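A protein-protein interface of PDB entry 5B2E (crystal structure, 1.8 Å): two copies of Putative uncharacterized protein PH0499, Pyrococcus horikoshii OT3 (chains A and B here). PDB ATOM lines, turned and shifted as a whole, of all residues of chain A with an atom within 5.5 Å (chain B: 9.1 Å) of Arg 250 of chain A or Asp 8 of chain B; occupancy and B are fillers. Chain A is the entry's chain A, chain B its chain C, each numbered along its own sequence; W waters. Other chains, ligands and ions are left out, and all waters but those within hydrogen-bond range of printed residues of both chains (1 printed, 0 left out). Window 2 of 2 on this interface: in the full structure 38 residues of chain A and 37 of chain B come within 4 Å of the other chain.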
ATOM      1  N   ASP A 205      19.774  -5.232  24.869  1.00  0.00           N
ATOM      2  CA  ASP A 205      19.235  -3.891  24.574  1.00  0.00           C
ATOM      3  C   ASP A 205      19.604  -3.503  23.134  1.00  0.00           C
ATOM      4  O   ASP A 205      20.809  -3.335  22.795  1.00  0.00           O
ATOM      5  CB  ASP A 205      19.873  -2.854  25.527  1.00  0.00           C
ATOM      6  CG  ASP A 205      19.375  -1.443  25.295  1.00  0.00           C
ATOM      7  OD1 ASP A 205      18.548  -1.150  24.370  1.00  0.00           O
ATOM      8  OD2 ASP A 205      19.816  -0.585  26.064  1.00  0.00           O
ATOM      9  N   THR A 207      17.968  -0.596  21.675  1.00  0.00           N
ATOM     10  CA  THR A 207      17.304   0.709  21.463  1.00  0.00           C
ATOM     11  C   THR A 207      18.094   1.580  20.486  1.00  0.00           C
ATOM     12  O   THR A 207      17.544   2.098  19.581  1.00  0.00           O
ATOM     13  CB  THR A 207      17.228   1.401  22.854  1.00  0.00           C
ATOM     14  OG1 THR A 207      16.396   0.543  23.679  1.00  0.00           O
ATOM     15  CG2 THR A 207      16.628   2.822  22.725  1.00  0.00           C
ATOM     16  N   ALA A 240       9.980  -5.753  19.369  1.00  0.00           N
ATOM     17  CA  ALA A 240      11.136  -5.288  20.143  1.00  0.00           C
ATOM     18  C   ALA A 240      10.794  -4.649  21.532  1.00  0.00           C
ATOM     19  O   ALA A 240      11.624  -4.737  22.490  1.00  0.00           O
ATOM     20  CB  ALA A 240      12.007  -4.325  19.336  1.00  0.00           C
ATOM     21  N   MET A 241       9.653  -3.947  21.647  1.00  0.00           N
ATOM     22  CA  MET A 241       9.233  -3.393  22.894  1.00  0.00           C
ATOM     23  C   MET A 241       8.854  -4.457  23.873  1.00  0.00           C
ATOM     24  O   MET A 241       9.116  -4.269  25.075  1.00  0.00           O
ATOM     25  CB  MET A 241       8.046  -2.395  22.761  1.00  0.00           C
ATOM     26  CG  MET A 241       8.430  -1.200  21.852  1.00  0.00           C
ATOM     27  SD  MET A 241       7.149   0.041  21.837  1.00  0.00           S
ATOM     28  CE  MET A 241       7.474   0.943  23.318  1.00  0.00           C
ATOM     29  N   GLY A 244      12.316  -5.477  25.060  1.00  0.00           N
ATOM     30  CA  GLY A 244      12.894  -4.375  25.762  1.00  0.00           C
ATOM     31  C   GLY A 244      12.345  -4.138  27.181  1.00  0.00           C
ATOM     32  O   GLY A 244      13.092  -3.935  28.130  1.00  0.00           O
ATOM     33  N   GLU A 245      11.021  -4.201  27.320  1.00  0.00           N
ATOM     34  CA  GLU A 245      10.392  -3.839  28.540  1.00  0.00           C
ATOM     35  C   GLU A 245      10.961  -4.702  29.681  1.00  0.00           C
ATOM     36  O   GLU A 245      11.030  -4.247  30.876  1.00  0.00           O
ATOM     37  CB  GLU A 245       8.865  -4.110  28.410  1.00  0.00           C
ATOM     38  CG  GLU A 245       8.128  -3.844  29.770  1.00  0.00           C
ATOM     39  CD  GLU A 245       6.629  -4.087  29.694  1.00  0.00           C
ATOM     40  OE1 GLU A 245       6.147  -4.787  28.739  1.00  0.00           O
ATOM     41  OE2 GLU A 245       5.927  -3.529  30.601  1.00  0.00           O
ATOM     42  N   GLY A 248      13.766  -3.071  31.064  1.00  0.00           N
ATOM     43  CA  GLY A 248      13.448  -1.641  31.226  1.00  0.00           C
ATOM     44  C   GLY A 248      14.090  -0.757  30.158  1.00  0.00           C
ATOM     45  O   GLY A 248      14.578   0.341  30.480  1.00  0.00           O
ATOM     46  N   VAL A 249      14.146  -1.238  28.898  1.00  0.00           N
ATOM     47  CA  VAL A 249      14.639  -0.416  27.793  1.00  0.00           C
ATOM     48  C   VAL A 249      13.557  -0.376  26.714  1.00  0.00           C
ATOM     49  O   VAL A 249      12.586  -1.116  26.772  1.00  0.00           O
ATOM     50  CB  VAL A 249      15.986  -0.880  27.199  1.00  0.00           C
ATOM     51  CG1 VAL A 249      17.072  -0.954  28.301  1.00  0.00           C
ATOM     52  CG2 VAL A 249      15.860  -2.247  26.470  1.00  0.00           C
ATOM     53  N   ARG A 250      13.741   0.493  25.738  1.00  0.00           N
ATOM     54  CA  ARG A 250      12.627   0.692  24.823  1.00  0.00           C
ATOM     55  C   ARG A 250      12.546  -0.551  23.880  1.00  0.00           C
ATOM     56  O   ARG A 250      11.464  -1.075  23.600  1.00  0.00           O
ATOM     57  CB  ARG A 250      12.875   1.962  24.010  1.00  0.00           C
ATOM     58  CG  ARG A 250      11.797   2.239  23.002  1.00  0.00           C
ATOM     59  CD  ARG A 250      12.026   3.632  22.338  1.00  0.00           C
ATOM     60  NE  ARG A 250      10.921   3.951  21.412  1.00  0.00           N
ATOM     61  CZ  ARG A 250       9.661   4.184  21.784  1.00  0.00           C
ATOM     62  NH1 ARG A 250       8.749   4.423  20.857  1.00  0.00           N
ATOM     63  NH2 ARG A 250       9.295   4.142  23.079  1.00  0.00           N
ATOM     64  N   TYR A 251      13.685  -0.961  23.340  1.00  0.00           N
ATOM     65  CA  TYR A 251      13.744  -2.043  22.311  1.00  0.00           C
ATOM     66  C   TYR A 251      14.796  -3.074  22.648  1.00  0.00           C
ATOM     67  O   TYR A 251      15.984  -2.739  22.902  1.00  0.00           O
ATOM     68  CB  TYR A 251      14.103  -1.493  20.898  1.00  0.00           C
ATOM     69  CG  TYR A 251      13.102  -0.542  20.285  1.00  0.00           C
ATOM     70  CD1 TYR A 251      11.756  -0.871  20.209  1.00  0.00           C
ATOM     71  CD2 TYR A 251      13.500   0.725  19.822  1.00  0.00           C
ATOM     72  CE1 TYR A 251      10.834   0.032  19.612  1.00  0.00           C
ATOM     73  CE2 TYR A 251      12.579   1.626  19.217  1.00  0.00           C
ATOM     74  CZ  TYR A 251      11.261   1.270  19.141  1.00  0.00           C
ATOM     75  OH  TYR A 251      10.384   2.167  18.595  1.00  0.00           O
ATOM     76  N   GLY A 252      14.387  -4.344  22.644  1.00  0.00           N
ATOM     77  CA  GLY A 252      15.338  -5.424  22.840  1.00  0.00           C
ATOM     78  C   GLY A 252      15.105  -6.592  21.899  1.00  0.00           C
ATOM     79  O   GLY A 252      14.149  -6.658  21.099  1.00  0.00           O
ATOM     80  N   PHE B   6       4.616   5.580  15.514  1.00  0.00           N
ATOM     81  CA  PHE B   6       4.915   4.297  16.250  1.00  0.00           C
ATOM     82  C   PHE B   6       6.258   4.330  16.975  1.00  0.00           C
ATOM     83  O   PHE B   6       6.359   3.907  18.136  1.00  0.00           O
ATOM     84  CB  PHE B   6       4.865   3.064  15.361  1.00  0.00           C
ATOM     85  CG  PHE B   6       3.889   2.002  15.858  1.00  0.00           C
ATOM     86  CD1 PHE B   6       4.295   1.035  16.743  1.00  0.00           C
ATOM     87  CD2 PHE B   6       2.592   1.991  15.399  1.00  0.00           C
ATOM     88  CE1 PHE B   6       3.386   0.062  17.232  1.00  0.00           C
ATOM     89  CE2 PHE B   6       1.648   1.027  15.864  1.00  0.00           C
ATOM     90  CZ  PHE B   6       2.055   0.077  16.792  1.00  0.00           C
ATOM     91  N   GLU B   7       7.271   4.847  16.290  1.00  0.00           N
ATOM     92  CA  GLU B   7       8.557   5.144  16.906  1.00  0.00           C
ATOM     93  C   GLU B   7       8.382   6.087  18.117  1.00  0.00           C
ATOM     94  O   GLU B   7       9.274   6.174  18.949  1.00  0.00           O
ATOM     95  CB  GLU B   7       9.520   5.773  15.881  1.00  0.00           C
ATOM     96  CG  GLU B   7       9.051   7.103  15.368  1.00  0.00           C
ATOM     97  CD  GLU B   7       8.536   7.053  13.944  1.00  0.00           C
ATOM     98  OE1 GLU B   7       7.593   6.260  13.662  1.00  0.00           O
ATOM     99  OE2 GLU B   7       9.069   7.835  13.119  1.00  0.00           O
ATOM    100  N   ASP B   8       7.216   6.739  18.216  1.00  0.00           N
ATOM    101  CA  ASP B   8       6.887   7.674  19.316  1.00  0.00           C
ATOM    102  C   ASP B   8       6.049   7.018  20.459  1.00  0.00           C
ATOM    103  O   ASP B   8       5.930   7.595  21.546  1.00  0.00           O
ATOM    104  CB  ASP B   8       6.125   8.907  18.759  1.00  0.00           C
ATOM    105  CG  ASP B   8       6.897   9.655  17.606  1.00  0.00           C
ATOM    106  OD1 ASP B   8       8.152   9.780  17.657  1.00  0.00           O
ATOM    107  OD2 ASP B   8       6.231  10.133  16.644  1.00  0.00           O
ATOM    108  N   ILE B   9       5.473   5.835  20.236  1.00  0.00           N
ATOM    109  CA  ILE B   9       4.717   5.171  21.318  1.00  0.00           C
ATOM    110  C   ILE B   9       5.594   4.914  22.545  1.00  0.00           C
ATOM    111  O   ILE B   9       6.763   4.477  22.411  1.00  0.00           O
ATOM    112  CB  ILE B   9       4.094   3.811  20.887  1.00  0.00           C
ATOM    113  CG1 ILE B   9       3.333   3.907  19.549  1.00  0.00           C
ATOM    114  CG2 ILE B   9       3.203   3.256  22.013  1.00  0.00           C
ATOM    115  CD1 ILE B   9       2.367   5.045  19.439  1.00  0.00           C
ATOM    116  N   ASP B  10       5.021   5.143  23.726  1.00  0.00           N
ATOM    117  CA  ASP B  10       5.762   5.064  24.983  1.00  0.00           C
ATOM    118  C   ASP B  10       6.062   3.668  25.552  1.00  0.00           C
ATOM    119  O   ASP B  10       7.180   3.402  25.985  1.00  0.00           O
ATOM    120  CB  ASP B  10       5.053   5.867  26.074  1.00  0.00           C
ATOM    121  CG  ASP B  10       5.419   7.345  26.066  1.00  0.00           C
ATOM    122  OD1 ASP B  10       4.499   8.157  26.359  1.00  0.00           O
ATOM    123  OD2 ASP B  10       6.604   7.702  25.780  1.00  0.00           O
ATOM    124  N   THR B  11       5.044   2.810  25.627  1.00  0.00           N
ATOM    125  CA  THR B  11       5.185   1.520  26.311  1.00  0.00           C
ATOM    126  C   THR B  11       4.791   0.402  25.375  1.00  0.00           C
ATOM    127  O   THR B  11       4.069   0.641  24.353  1.00  0.00           O
ATOM    128  CB  THR B  11       4.275   1.429  27.559  1.00  0.00           C
ATOM    129  OG1 THR B  11       2.912   1.586  27.132  1.00  0.00           O
ATOM    130  CG2 THR B  11       4.642   2.531  28.563  1.00  0.00           C
ATOM    131  N   PHE B  12       5.284  -0.783  25.685  1.00  0.00           N
ATOM    132  CA  PHE B  12       4.879  -1.986  24.984  1.00  0.00           C
ATOM    133  C   PHE B  12       3.346  -2.117  25.028  1.00  0.00           C
ATOM    134  O   PHE B  12       2.704  -2.419  24.014  1.00  0.00           O
ATOM    135  CB  PHE B  12       5.530  -3.258  25.542  1.00  0.00           C
ATOM    136  CG  PHE B  12       4.814  -4.491  25.098  1.00  0.00           C
ATOM    137  CD1 PHE B  12       4.856  -4.870  23.733  1.00  0.00           C
ATOM    138  CD2 PHE B  12       4.012  -5.204  25.982  1.00  0.00           C
ATOM    139  CE1 PHE B  12       4.130  -5.961  23.302  1.00  0.00           C
ATOM    140  CE2 PHE B  12       3.304  -6.307  25.568  1.00  0.00           C
ATOM    141  CZ  PHE B  12       3.360  -6.706  24.223  1.00  0.00           C
ATOM    142  N   GLU B  14       0.942   0.027  25.174  1.00  0.00           N
ATOM    143  CA  GLU B  14       0.332   0.932  24.203  1.00  0.00           C
ATOM    144  C   GLU B  14       0.573   0.517  22.776  1.00  0.00           C
ATOM    145  O   GLU B  14      -0.358   0.579  21.955  1.00  0.00           O
ATOM    146  CB  GLU B  14       0.807   2.392  24.375  1.00  0.00           C
ATOM    147  CG  GLU B  14       0.408   3.022  25.749  1.00  0.00           C
ATOM    148  CD  GLU B  14       1.289   4.270  26.127  1.00  0.00           C
ATOM    149  OE1 GLU B  14       2.235   4.653  25.381  1.00  0.00           O
ATOM    150  OE2 GLU B  14       1.022   4.866  27.179  1.00  0.00           O
ATOM    151  N   ALA B  15       1.825   0.144  22.471  1.00  0.00           N
ATOM    152  CA  ALA B  15       2.154  -0.375  21.099  1.00  0.00           C
ATOM    153  C   ALA B  15       1.344  -1.594  20.715  1.00  0.00           C
ATOM    154  O   ALA B  15       0.806  -1.654  19.621  1.00  0.00           O
ATOM    155  CB  ALA B  15       3.595  -0.731  21.038  1.00  0.00           C
ATOM    156  N   LYS B  18      -2.298  -0.497  19.876  1.00  0.00           N
ATOM    157  CA  LYS B  18      -2.359   0.165  18.601  1.00  0.00           C
ATOM    158  C   LYS B  18      -2.104  -0.804  17.464  1.00  0.00           C
ATOM    159  O   LYS B  18      -2.723  -0.684  16.388  1.00  0.00           O
ATOM    160  CB  LYS B  18      -1.284   1.263  18.527  1.00  0.00           C
ATOM    161  CG  LYS B  18      -1.691   2.549  17.901  1.00  0.00           C
ATOM    162  CD  LYS B  18      -1.493   3.668  18.968  1.00  0.00           C
ATOM    163  CE  LYS B  18      -1.954   5.025  18.470  1.00  0.00           C
ATOM    164  NZ  LYS B  18      -3.262   5.406  19.123  1.00  0.00           N
HETATM  165  O   HOH W   1       7.931   1.724  19.003  1.00  0.00           O
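The guanidinium group of Arg 250 of chain A lies within hydrogen-bond range of the backbone carbonyl oxygen of Glu 7 of chain B (2.6 Å).
The backbone carbonyl oxygen (O) of Ile 9 of chain B lies within hydrogen-bond range of the guanidinium group (NH1) of Arg 250 of chain A (2.5 Å).
N of Asp 10 of chain B lies close to OE1 of Glu 14 of chain B, at 3.3 Å.
OG1 of Thr 207 of chain A lies within hydrogen-bond range of N of Arg 250 of chain A (3.4 Å).
The backbone NH of Glu 14 of chain B is in hydrogen-bond range of the side-chain hydroxyl of Thr 11 of chain B (3.2 Å).
The side-chain hydroxyl (OG1) of Thr 207 of chain A sits at hydrogen-bond distance from the backbone NH (N) of Tyr 251 of chain A, 3.1 Å away.
The side-chain hydroxyl of Tyr 251 of chain A is in hydrogen-bond range of the guanidinium group of Arg 250 of chain A, 3.4 Å away.
Met 241 of chain A touches Ile 9 of chain B.
Met 241 of chain A touches Asp 10 of chain B (CE to O, 3.6 Å).
Met 241 of chain A touches Thr 11 of chain B (CE to C, 3.4 Å).
Met 241 of chain A touches Phe 12 of chain B (CE to N, 3.7 Å).
Met 241 of chain A touches Ala 15 of chain B (SD to CB, 3.7 Å).
Glu 245 of chain A touches Phe 12 of chain B (OE1 to CD2, 3.5 Å).
NH1 of Arg 250 of chain A touches O of Phe 6 of chain B, 3.7 Å away.
NH1 of Arg 250 of chain A touches C of Asp 8 of chain B (3.8 Å).
O of Asp 10 of chain B touches NH2 of Arg 250 of chain A, 3.7 Å away.
Tyr 251 of chain A touches Glu 7 of chain B (OH to CA, 3.9 Å).
Of the printed residues of chain B, Glu 245 of chain A touches Phe 12 (3.5 Å).
Of chain B, only Phe 6 (3.7 Å), Glu 7 (2.6 Å), Asp 8 (3.8 Å), Ile 9 (2.5 Å) and Asp 10 (3.7 Å) come within 4 Å of Arg 250 of chain A.
Tyr 251 of chain A touches just one residue of chain B: Glu 7 (3.9 Å).
Of the printed residues of chain A, Glu 7 of chain B touches Arg 250 and Tyr 251.
Of chain A, only Arg 250 (3.8 Å) comes within 4 Å of Asp 8 of chain B.
Printed residues of chain A within 4 Å of Thr 11 of chain B: Met 241.
Printed residues of chain A within 4 Å of Phe 12 of chain B: Met 241 (3.7 Å) and Glu 245 (3.5 Å).
Printed residues of chain A within 4 Å of Ala 15 of chain B: Met 241.
The nearest printed residue of chain A that does not touch Asp 8 of chain B is Tyr 251 of chain A (5.6 Å).
The nearest printed residue of chain A that does not touch Phe 12 of chain B is Ala 240 of chain A (6.3 Å).
Of the 10 printed residues of chain B, 8 touch a printed residue of chain A.
Hydrophobic or aromatic side chains of chain B that line the printed part of chain A: Phe 12 and Ala 15.
Among the printed residues, 12 pairs touch across the chains.
No position is printed for both chains.
Water W1 lies within hydrogen-bond range of OH of Tyr 251 of chain A, O of Phe 6 of chain B, NH1 of Arg 250 of chain A and SD of Met 241 of chain A.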
